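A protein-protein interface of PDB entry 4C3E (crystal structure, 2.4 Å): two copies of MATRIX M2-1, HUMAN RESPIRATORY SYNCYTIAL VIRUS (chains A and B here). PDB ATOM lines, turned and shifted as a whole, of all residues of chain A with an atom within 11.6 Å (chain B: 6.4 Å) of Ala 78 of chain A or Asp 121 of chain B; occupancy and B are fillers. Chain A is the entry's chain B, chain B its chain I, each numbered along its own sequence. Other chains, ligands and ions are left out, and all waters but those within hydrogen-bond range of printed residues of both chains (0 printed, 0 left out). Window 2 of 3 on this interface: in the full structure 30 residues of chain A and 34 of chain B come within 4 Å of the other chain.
O of Asp 72 of chain A lies within hydrogen-bond range of NH2 of Arg 120 of chain B (2.4 Å).
OD1 of Asp 72 of chain A is in salt-bridge range of NZ of Lys 117 of chain B, 2.8 Å away.
O of Thr 74 of chain A sits close to OD1 of Asp 121 of chain B.
The guanidinium group (NH2) of Arg 73 of chain A lies within salt-bridge range of the side-chain carboxylate (OE2) of Glu 76 of chain A.
The side-chain amide oxygen (OD1) of Asn 122 of chain B sits close to the backbone carbonyl oxygen (O) of Lys 118 of chain B (3.5 Å).
Among the printed residues, pairs that only touch across the chains: Tyr 77 of chain A with Lys 118 of chain B, Thr 74 of chain A with Arg 120 of chain B, Arg 73 of chain A with Arg 120 of chain B, Tyr 77 of chain A with Lys 117 of chain B and Ala 78 of chain A with Asp 121 of chain B.
Printed residues of chain B within 4 Å of Asp 72 of chain A: Lys 117 (2.8 Å) and Arg 120 (2.4 Å).
Of the printed residues of chain B, Thr 74 of chain A touches Arg 120 and Asp 121.
Of the printed residues of chain B, Tyr 77 of chain A touches Lys 117 and Lys 118.
Printed residues of chain B within 4 Å of Ala 78 of chain A: Asp 121.
Printed residues of chain A within 4 Å of Lys 117 of chain B: Asp 72 (2.8 Å) and Tyr 77 (3.7 Å).
Asn 122 of chain B touches none of the printed residues of chain A.
The nearest printed residue of chain B that does not touch Ala 78 of chain A is Arg 120 of chain B (7.1 Å).
The nearest printed residue of chain A that does not touch Asp 121 of chain B is Tyr 77 of chain A (4.01 Å).
Printed residues of chain B that touch a printed residue of chain A: Lys 117, Lys 118, Arg 120 and Asp 121.
Of the 22 printed residues of chain A, 5 touch a printed residue of chain B.
Printed residues of chain A that touch a printed residue of chain B: Asp 72, Arg 73, Thr 74, Tyr 77 and Ala 78.
Along chain A the printed residues that touch a printed residue of chain B span positions 72 to 78.
Among the printed residues, 8 pairs touch across the chains.
No position is printed for both chains.
Of the 8 pairs that touch across the chains among the printed residues, none has its exchanged pair printed and touching as well.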
ATOM      1  N   ALA A  69      -9.608  12.695 -13.444  1.00  0.00           N
ATOM      2  CA  ALA A  69     -10.781  11.863 -13.792  1.00  0.00           C
ATOM      3  C   ALA A  69     -10.712  11.364 -15.242  1.00  0.00           C
ATOM      4  O   ALA A  69     -11.111  10.228 -15.545  1.00  0.00           O
ATOM      5  CB  ALA A  69     -12.071  12.641 -13.549  1.00  0.00           C
ATOM      6  N   GLU A  70     -10.154  12.210 -16.109  1.00  0.00           N
ATOM      7  CA  GLU A  70      -9.917  11.881 -17.509  1.00  0.00           C
ATOM      8  C   GLU A  70      -9.093  10.599 -17.688  1.00  0.00           C
ATOM      9  O   GLU A  70      -9.349   9.820 -18.615  1.00  0.00           O
ATOM     10  CB  GLU A  70      -9.227  13.045 -18.246  1.00  0.00           C
ATOM     11  CG  GLU A  70     -10.125  14.247 -18.524  1.00  0.00           C
ATOM     12  CD  GLU A  70     -10.196  15.249 -17.366  1.00  0.00           C
ATOM     13  OE1 GLU A  70     -10.189  14.845 -16.180  1.00  0.00           O
ATOM     14  OE2 GLU A  70     -10.274  16.458 -17.648  1.00  0.00           O
ATOM     15  N   LEU A  71      -8.137  10.352 -16.792  1.00  0.00           N
ATOM     16  CA  LEU A  71      -7.296   9.128 -16.881  1.00  0.00           C
ATOM     17  C   LEU A  71      -8.056   7.805 -16.627  1.00  0.00           C
ATOM     18  O   LEU A  71      -7.551   6.739 -16.985  1.00  0.00           O
ATOM     19  CB  LEU A  71      -6.084   9.229 -15.950  1.00  0.00           C
ATOM     20  CG  LEU A  71      -5.158  10.434 -16.171  1.00  0.00           C
ATOM     21  CD1 LEU A  71      -4.030  10.387 -15.165  1.00  0.00           C
ATOM     22  CD2 LEU A  71      -4.606  10.479 -17.582  1.00  0.00           C
ATOM     23  N   ASP A  72      -9.270   7.902 -16.064  1.00  0.00           N
ATOM     24  CA  ASP A  72     -10.146   6.736 -15.794  1.00  0.00           C
ATOM     25  C   ASP A  72     -11.093   6.374 -16.944  1.00  0.00           C
ATOM     26  O   ASP A  72     -11.722   5.308 -16.907  1.00  0.00           O
ATOM     27  CB  ASP A  72     -10.988   6.961 -14.536  1.00  0.00           C
ATOM     28  CG  ASP A  72     -10.145   7.120 -13.272  1.00  0.00           C
ATOM     29  OD1 ASP A  72      -9.076   6.482 -13.148  1.00  0.00           O
ATOM     30  OD2 ASP A  72     -10.563   7.898 -12.387  1.00  0.00           O
ATOM     31  N   ARG A  73     -11.196   7.259 -17.943  1.00  0.00           N
ATOM     32  CA  ARG A  73     -12.044   7.038 -19.126  1.00  0.00           C
ATOM     33  C   ARG A  73     -11.493   5.936 -20.020  1.00  0.00           C
ATOM     34  O   ARG A  73     -10.354   5.527 -19.885  1.00  0.00           O
ATOM     35  CB  ARG A  73     -12.190   8.318 -19.930  1.00  0.00           C
ATOM     36  CG  ARG A  73     -13.250   9.248 -19.356  1.00  0.00           C
ATOM     37  CD  ARG A  73     -13.005  10.727 -19.647  1.00  0.00           C
ATOM     38  NE  ARG A  73     -12.167  10.974 -20.830  1.00  0.00           N
ATOM     39  CZ  ARG A  73     -11.876  12.184 -21.287  1.00  0.00           C
ATOM     40  NH1 ARG A  73     -12.362  13.266 -20.686  1.00  0.00           N
ATOM     41  NH2 ARG A  73     -11.108  12.318 -22.353  1.00  0.00           N
ATOM     42  N   THR A  74     -12.331   5.459 -20.928  1.00  0.00           N
ATOM     43  CA  THR A  74     -12.068   4.240 -21.685  1.00  0.00           C
ATOM     44  C   THR A  74     -10.762   4.287 -22.485  1.00  0.00           C
ATOM     45  O   THR A  74     -10.032   3.288 -22.518  1.00  0.00           O
ATOM     46  CB  THR A  74     -13.266   3.896 -22.618  1.00  0.00           C
ATOM     47  OG1 THR A  74     -14.372   3.476 -21.813  1.00  0.00           O
ATOM     48  CG2 THR A  74     -12.939   2.756 -23.593  1.00  0.00           C
ATOM     49  N   GLU A  75     -10.470   5.411 -23.138  1.00  0.00           N
ATOM     50  CA  GLU A  75      -9.327   5.416 -24.055  1.00  0.00           C
ATOM     51  C   GLU A  75      -7.971   5.701 -23.337  1.00  0.00           C
ATOM     52  O   GLU A  75      -6.933   5.270 -23.782  1.00  0.00           O
ATOM     53  CB  GLU A  75      -9.610   6.293 -25.286  1.00  0.00           C
ATOM     54  CG  GLU A  75      -9.032   7.699 -25.318  1.00  0.00           C
ATOM     55  CD  GLU A  75      -8.888   8.216 -26.752  1.00  0.00           C
ATOM     56  OE1 GLU A  75      -9.612   7.730 -27.662  1.00  0.00           O
ATOM     57  OE2 GLU A  75      -8.029   9.095 -26.984  1.00  0.00           O
ATOM     58  N   GLU A  76      -8.030   6.370 -22.198  1.00  0.00           N
ATOM     59  CA  GLU A  76      -6.856   6.700 -21.427  1.00  0.00           C
ATOM     60  C   GLU A  76      -6.464   5.451 -20.650  1.00  0.00           C
ATOM     61  O   GLU A  76      -5.287   5.175 -20.448  1.00  0.00           O
ATOM     62  CB  GLU A  76      -7.130   7.942 -20.575  1.00  0.00           C
ATOM     63  CG  GLU A  76      -8.246   8.780 -21.245  1.00  0.00           C
ATOM     64  CD  GLU A  76      -7.995  10.264 -21.398  1.00  0.00           C
ATOM     65  OE1 GLU A  76      -7.100  10.834 -20.729  1.00  0.00           O
ATOM     66  OE2 GLU A  76      -8.739  10.870 -22.201  1.00  0.00           O
ATOM     67  N   TYR A  77      -7.456   4.649 -20.297  1.00  0.00           N
ATOM     68  CA  TYR A  77      -7.218   3.341 -19.698  1.00  0.00           C
ATOM     69  C   TYR A  77      -6.530   2.418 -20.690  1.00  0.00           C
ATOM     70  O   TYR A  77      -5.678   1.627 -20.321  1.00  0.00           O
ATOM     71  CB  TYR A  77      -8.549   2.697 -19.157  1.00  0.00           C
ATOM     72  CG  TYR A  77      -8.383   1.235 -18.743  1.00  0.00           C
ATOM     73  CD1 TYR A  77      -7.901   0.895 -17.475  1.00  0.00           C
ATOM     74  CD2 TYR A  77      -8.626   0.213 -19.651  1.00  0.00           C
ATOM     75  CE1 TYR A  77      -7.695  -0.436 -17.111  1.00  0.00           C
ATOM     76  CE2 TYR A  77      -8.452  -1.116 -19.311  1.00  0.00           C
ATOM     77  CZ  TYR A  77      -7.980  -1.438 -18.040  1.00  0.00           C
ATOM     78  OH  TYR A  77      -7.801  -2.764 -17.723  1.00  0.00           O
ATOM     79  N   ALA A  78      -6.897   2.512 -21.959  1.00  0.00           N
ATOM     80  CA  ALA A  78      -6.282   1.653 -22.967  1.00  0.00           C
ATOM     81  C   ALA A  78      -4.878   2.090 -23.301  1.00  0.00           C
ATOM     82  O   ALA A  78      -4.027   1.274 -23.673  1.00  0.00           O
ATOM     83  CB  ALA A  78      -7.133   1.647 -24.238  1.00  0.00           C
ATOM     84  N   LEU A  79      -4.661   3.397 -23.222  1.00  0.00           N
ATOM     85  CA  LEU A  79      -3.348   3.989 -23.497  1.00  0.00           C
ATOM     86  C   LEU A  79      -2.366   3.669 -22.353  1.00  0.00           C
ATOM     87  O   LEU A  79      -1.210   3.377 -22.577  1.00  0.00           O
ATOM     88  CB  LEU A  79      -3.471   5.500 -23.572  1.00  0.00           C
ATOM     89  CG  LEU A  79      -4.013   6.042 -24.910  1.00  0.00           C
ATOM     90  CD1 LEU A  79      -4.295   7.536 -24.756  1.00  0.00           C
ATOM     91  CD2 LEU A  79      -3.039   5.793 -26.037  1.00  0.00           C
ATOM     92  N   GLY A  80      -2.893   3.686 -21.138  1.00  0.00           N
ATOM     93  CA  GLY A  80      -2.099   3.545 -19.949  1.00  0.00           C
ATOM     94  C   GLY A  80      -1.500   4.863 -19.682  1.00  0.00           C
ATOM     95  O   GLY A  80      -1.474   5.723 -20.538  1.00  0.00           O
ATOM     96  N   VAL A  81      -0.904   4.977 -18.516  1.00  0.00           N
ATOM     97  CA  VAL A  81      -0.122   6.153 -18.192  1.00  0.00           C
ATOM     98  C   VAL A  81       0.965   6.461 -19.245  1.00  0.00           C
ATOM     99  O   VAL A  81       1.216   7.588 -19.517  1.00  0.00           O
ATOM    100  CB  VAL A  81       0.482   5.975 -16.791  1.00  0.00           C
ATOM    101  CG1 VAL A  81       1.592   6.954 -16.489  1.00  0.00           C
ATOM    102  CG2 VAL A  81      -0.634   6.159 -15.769  1.00  0.00           C
ATOM    103  N   VAL A  82       1.669   5.457 -19.734  1.00  0.00           N
ATOM    104  CA  VAL A  82       2.763   5.675 -20.647  1.00  0.00           C
ATOM    105  C   VAL A  82       2.200   6.151 -21.991  1.00  0.00           C
ATOM    106  O   VAL A  82       2.678   7.123 -22.532  1.00  0.00           O
ATOM    107  CB  VAL A  82       3.582   4.402 -20.838  1.00  0.00           C
ATOM    108  CG1 VAL A  82       4.510   4.513 -22.050  1.00  0.00           C
ATOM    109  CG2 VAL A  82       4.418   4.130 -19.563  1.00  0.00           C
ATOM    110  N   GLY A  83       1.139   5.509 -22.479  1.00  0.00           N
ATOM    111  CA  GLY A  83       0.422   5.973 -23.688  1.00  0.00           C
ATOM    112  C   GLY A  83      -0.086   7.401 -23.549  1.00  0.00           C
ATOM    113  O   GLY A  83       0.071   8.211 -24.434  1.00  0.00           O
ATOM    114  N   VAL A  84      -0.621   7.722 -22.414  1.00  0.00           N
ATOM    115  CA  VAL A  84      -1.095   9.060 -22.168  1.00  0.00           C
ATOM    116  C   VAL A  84       0.071  10.039 -22.270  1.00  0.00           C
ATOM    117  O   VAL A  84      -0.068  11.069 -22.879  1.00  0.00           O
ATOM    118  CB  VAL A  84      -1.724   9.159 -20.797  1.00  0.00           C
ATOM    119  CG1 VAL A  84      -1.924  10.612 -20.367  1.00  0.00           C
ATOM    120  CG2 VAL A  84      -3.101   8.477 -20.813  1.00  0.00           C
ATOM    121  N   LEU A  85       1.233   9.691 -21.699  1.00  0.00           N
ATOM    122  CA  LEU A  85       2.346  10.608 -21.688  1.00  0.00           C
ATOM    123  C   LEU A  85       2.971  10.732 -23.090  1.00  0.00           C
ATOM    124  O   LEU A  85       3.332  11.816 -23.472  1.00  0.00           O
ATOM    125  CB  LEU A  85       3.409  10.195 -20.683  1.00  0.00           C
ATOM    126  CG  LEU A  85       2.978  10.344 -19.255  1.00  0.00           C
ATOM    127  CD1 LEU A  85       3.908   9.553 -18.358  1.00  0.00           C
ATOM    128  CD2 LEU A  85       2.885  11.757 -18.801  1.00  0.00           C
ATOM    129  N   GLU A  86       3.122   9.619 -23.793  1.00  0.00           N
ATOM    130  CA  GLU A  86       3.658   9.608 -25.121  1.00  0.00           C
ATOM    131  C   GLU A  86       2.717  10.384 -26.078  1.00  0.00           C
ATOM    132  O   GLU A  86       3.183  11.078 -26.977  1.00  0.00           O
ATOM    133  CB  GLU A  86       3.860   8.182 -25.614  1.00  0.00           C
ATOM    134  CG  GLU A  86       5.049   7.479 -24.959  1.00  0.00           C
ATOM    135  CD  GLU A  86       5.299   6.048 -25.413  1.00  0.00           C
ATOM    136  OE1 GLU A  86       4.480   5.444 -26.116  1.00  0.00           O
ATOM    137  OE2 GLU A  86       6.380   5.499 -25.074  1.00  0.00           O
ATOM    138  N   SER A  87       1.413  10.261 -25.857  1.00  0.00           N
ATOM    139  CA  SER A  87       0.409  10.974 -26.639  1.00  0.00           C
ATOM    140  C   SER A  87       0.478  12.467 -26.393  1.00  0.00           C
ATOM    141  O   SER A  87       0.440  13.239 -27.340  1.00  0.00           O
ATOM    142  CB  SER A  87      -1.004  10.472 -26.339  1.00  0.00           C
ATOM    143  OG  SER A  87      -1.192   9.191 -26.884  1.00  0.00           O
ATOM    144  N   ASN A  93      -4.372  12.106 -29.458  1.00  0.00           N
ATOM    145  CA  ASN A  93      -5.358  11.515 -28.544  1.00  0.00           C
ATOM    146  C   ASN A  93      -5.925  12.407 -27.480  1.00  0.00           C
ATOM    147  O   ASN A  93      -6.413  11.934 -26.443  1.00  0.00           O
ATOM    148  CB  ASN A  93      -4.773  10.258 -27.963  1.00  0.00           C
ATOM    149  CG  ASN A  93      -4.446   9.245 -29.055  1.00  0.00           C
ATOM    150  OD1 ASN A  93      -5.327   8.922 -29.834  1.00  0.00           O
ATOM    151  ND2 ASN A  93      -3.278   8.598 -28.982  1.00  0.00           N
ATOM    152  N   ILE A  95      -4.909  14.510 -25.174  1.00  0.00           N
ATOM    153  CA  ILE A  95      -4.403  14.557 -23.816  1.00  0.00           C
ATOM    154  C   ILE A  95      -4.088  15.989 -23.495  1.00  0.00           C
ATOM    155  O   ILE A  95      -3.255  16.614 -24.155  1.00  0.00           O
ATOM    156  CB  ILE A  95      -3.152  13.709 -23.674  1.00  0.00           C
ATOM    157  CG1 ILE A  95      -3.403  12.266 -24.165  1.00  0.00           C
ATOM    158  CG2 ILE A  95      -2.672  13.741 -22.256  1.00  0.00           C
ATOM    159  CD1 ILE A  95      -4.585  11.586 -23.506  1.00  0.00           C
ATOM    160  N   LYS A 106       1.817   9.662 -11.594  1.00  0.00           N
ATOM    161  CA  LYS A 106       1.670   8.218 -11.466  1.00  0.00           C
ATOM    162  C   LYS A 106       2.907   7.493 -11.895  1.00  0.00           C
ATOM    163  O   LYS A 106       3.205   6.436 -11.366  1.00  0.00           O
ATOM    164  CB  LYS A 106       0.473   7.720 -12.254  1.00  0.00           C
ATOM    165  CG  LYS A 106      -0.847   8.326 -11.777  1.00  0.00           C
ATOM    166  CD  LYS A 106      -1.932   7.280 -11.610  1.00  0.00           C
ATOM    167  CE  LYS A 106      -2.981   7.325 -12.693  1.00  0.00           C
ATOM    168  NZ  LYS A 106      -4.005   8.329 -12.307  1.00  0.00           N
ATOM    169  N   ILE B 116     -12.996  -3.805 -13.352  1.00  0.00           N
ATOM    170  CA  ILE B 116     -14.205  -3.361 -14.027  1.00  0.00           C
ATOM    171  C   ILE B 116     -13.822  -2.579 -15.284  1.00  0.00           C
ATOM    172  O   ILE B 116     -14.360  -2.833 -16.348  1.00  0.00           O
ATOM    173  CB  ILE B 116     -15.086  -2.424 -13.182  1.00  0.00           C
ATOM    174  CG1 ILE B 116     -15.159  -2.870 -11.714  1.00  0.00           C
ATOM    175  CG2 ILE B 116     -16.467  -2.316 -13.793  1.00  0.00           C
ATOM    176  CD1 ILE B 116     -16.167  -3.914 -11.419  1.00  0.00           C
ATOM    177  N   LYS B 117     -12.853  -1.658 -15.158  1.00  0.00           N
ATOM    178  CA  LYS B 117     -12.364  -0.933 -16.317  1.00  0.00           C
ATOM    179  C   LYS B 117     -11.966  -1.913 -17.402  1.00  0.00           C
ATOM    180  O   LYS B 117     -12.213  -1.654 -18.554  1.00  0.00           O
ATOM    181  CB  LYS B 117     -11.214   0.007 -15.962  1.00  0.00           C
ATOM    182  CG  LYS B 117     -11.702   1.164 -15.144  1.00  0.00           C
ATOM    183  CD  LYS B 117     -10.572   1.987 -14.613  1.00  0.00           C
ATOM    184  CE  LYS B 117     -11.130   3.009 -13.648  1.00  0.00           C
ATOM    185  NZ  LYS B 117     -10.030   3.816 -13.068  1.00  0.00           N
ATOM    186  N   LYS B 118     -11.322  -3.009 -17.035  1.00  0.00           N
ATOM    187  CA  LYS B 118     -10.942  -3.966 -18.036  1.00  0.00           C
ATOM    188  C   LYS B 118     -12.169  -4.525 -18.738  1.00  0.00           C
ATOM    189  O   LYS B 118     -12.150  -4.704 -19.954  1.00  0.00           O
ATOM    190  CB  LYS B 118     -10.071  -5.072 -17.470  1.00  0.00           C
ATOM    191  CG  LYS B 118      -9.826  -6.177 -18.483  1.00  0.00           C
ATOM    192  CD  LYS B 118      -8.682  -7.102 -18.103  1.00  0.00           C
ATOM    193  CE  LYS B 118      -8.536  -8.208 -19.153  1.00  0.00           C
ATOM    194  NZ  LYS B 118      -7.766  -9.386 -18.656  1.00  0.00           N
ATOM    195  N   LEU B 119     -13.241  -4.762 -18.003  1.00  0.00           N
ATOM    196  CA  LEU B 119     -14.469  -5.267 -18.622  1.00  0.00           C
ATOM    197  C   LEU B 119     -15.121  -4.213 -19.510  1.00  0.00           C
ATOM    198  O   LEU B 119     -15.580  -4.511 -20.606  1.00  0.00           O
ATOM    199  CB  LEU B 119     -15.502  -5.659 -17.579  1.00  0.00           C
ATOM    200  CG  LEU B 119     -15.206  -6.911 -16.767  1.00  0.00           C
ATOM    201  CD1 LEU B 119     -16.233  -7.008 -15.656  1.00  0.00           C
ATOM    202  CD2 LEU B 119     -15.218  -8.163 -17.630  1.00  0.00           C
ATOM    203  N   ARG B 120     -15.148  -2.982 -19.016  1.00  0.00           N
ATOM    204  CA  ARG B 120     -15.679  -1.874 -19.728  1.00  0.00           C
ATOM    205  C   ARG B 120     -14.998  -1.715 -21.103  1.00  0.00           C
ATOM    206  O   ARG B 120     -15.624  -1.299 -22.073  1.00  0.00           O
ATOM    207  CB  ARG B 120     -15.496  -0.626 -18.900  1.00  0.00           C
ATOM    208  CG  ARG B 120     -16.104   0.609 -19.520  1.00  0.00           C
ATOM    209  CD  ARG B 120     -15.926   1.807 -18.608  1.00  0.00           C
ATOM    210  NE  ARG B 120     -14.499   2.118 -18.528  1.00  0.00           N
ATOM    211  CZ  ARG B 120     -13.975   3.066 -17.778  1.00  0.00           C
ATOM    212  NH1 ARG B 120     -14.744   3.814 -16.984  1.00  0.00           N
ATOM    213  NH2 ARG B 120     -12.653   3.267 -17.829  1.00  0.00           N
ATOM    214  N   ASP B 121     -13.712  -1.997 -21.154  1.00  0.00           N
ATOM    215  CA  ASP B 121     -12.943  -1.828 -22.357  1.00  0.00           C
ATOM    216  C   ASP B 121     -13.248  -2.897 -23.406  1.00  0.00           C
ATOM    217  O   ASP B 121     -13.041  -2.656 -24.592  1.00  0.00           O
ATOM    218  CB  ASP B 121     -11.461  -1.878 -22.001  1.00  0.00           C
ATOM    219  CG  ASP B 121     -10.585  -1.346 -23.098  1.00  0.00           C
ATOM    220  OD1 ASP B 121     -10.469  -0.072 -23.197  1.00  0.00           O
ATOM    221  OD2 ASP B 121     -10.030  -2.219 -23.830  1.00  0.00           O
ATOM    222  N   ASN B 122     -13.737  -4.053 -22.986  1.00  0.00           N
ATOM    223  CA  ASN B 122     -14.208  -5.075 -23.934  1.00  0.00           C
ATOM    224  C   ASN B 122     -15.587  -4.784 -24.543  1.00  0.00           C
ATOM    225  O   ASN B 122     -15.980  -5.449 -25.483  1.00  0.00           O
ATOM    226  CB  ASN B 122     -14.298  -6.436 -23.285  1.00  0.00           C
ATOM    227  CG  ASN B 122     -12.959  -6.948 -22.803  1.00  0.00           C
ATOM    228  OD1 ASN B 122     -12.872  -7.596 -21.753  1.00  0.00           O
ATOM    229  ND2 ASN B 122     -11.907  -6.652 -23.546  1.00  0.00           N
ATOM    230  N   GLU B 123     -16.286  -3.759 -24.050  1.00  0.00           N
ATOM    231  CA  GLU B 123     -17.591  -3.407 -24.582  1.00  0.00           C
ATOM    232  C   GLU B 123     -17.501  -2.533 -25.824  1.00  0.00           C
ATOM    233  O   GLU B 123     -16.668  -1.614 -25.898  1.00  0.00           O
ATOM    234  CB  GLU B 123     -18.422  -2.656 -23.527  1.00  0.00           C
ATOM    235  CG  GLU B 123     -18.997  -3.570 -22.428  1.00  0.00           C
ATOM    236  CD  GLU B 123     -19.827  -4.716 -22.969  1.00  0.00           C
ATOM    237  OE1 GLU B 123     -20.868  -4.445 -23.647  1.00  0.00           O
ATOM    238  OE2 GLU B 123     -19.389  -5.875 -22.827  1.00  0.00           O
ATOM    239  N   GLU B 124     -18.384  -2.815 -26.782  1.00  0.00           N
ATOM    240  CA  GLU B 124     -18.605  -1.959 -27.944  1.00  0.00           C
ATOM    241  C   GLU B 124     -19.121  -0.636 -27.419  1.00  0.00           C
ATOM    242  O   GLU B 124     -19.800  -0.624 -26.387  1.00  0.00           O
ATOM    243  CB  GLU B 124     -19.630  -2.600 -28.907  1.00  0.00           C
ATOM    244  CG  GLU B 124     -19.258  -3.973 -29.493  1.00  0.00           C
ATOM    245  CD  GLU B 124     -18.216  -3.902 -30.616  1.00  0.00           C
ATOM    246  OE1 GLU B 124     -18.330  -3.035 -31.518  1.00  0.00           O
ATOM    247  OE2 GLU B 124     -17.282  -4.732 -30.623  1.00  0.00           O
ATOM    248  N   TYR B 133     -21.226  -0.578 -15.462  1.00  0.00           N
ATOM    249  CA  TYR B 133     -19.822  -0.574 -15.083  1.00  0.00           C
ATOM    250  C   TYR B 133     -19.394   0.738 -14.468  1.00  0.00           C
ATOM    251  O   TYR B 133     -18.775   0.742 -13.406  1.00  0.00           O
ATOM    252  CB  TYR B 133     -18.935  -0.899 -16.246  1.00  0.00           C
ATOM    253  CG  TYR B 133     -19.032  -2.312 -16.770  1.00  0.00           C
ATOM    254  CD1 TYR B 133     -19.352  -3.383 -15.962  1.00  0.00           C
ATOM    255  CD2 TYR B 133     -18.802  -2.572 -18.104  1.00  0.00           C
ATOM    256  CE1 TYR B 133     -19.388  -4.678 -16.469  1.00  0.00           C
ATOM    257  CE2 TYR B 133     -18.850  -3.857 -18.618  1.00  0.00           C
ATOM    258  CZ  TYR B 133     -19.133  -4.903 -17.788  1.00  0.00           C
ATOM    259  OH  TYR B 133     -19.134  -6.170 -18.288  1.00  0.00           O
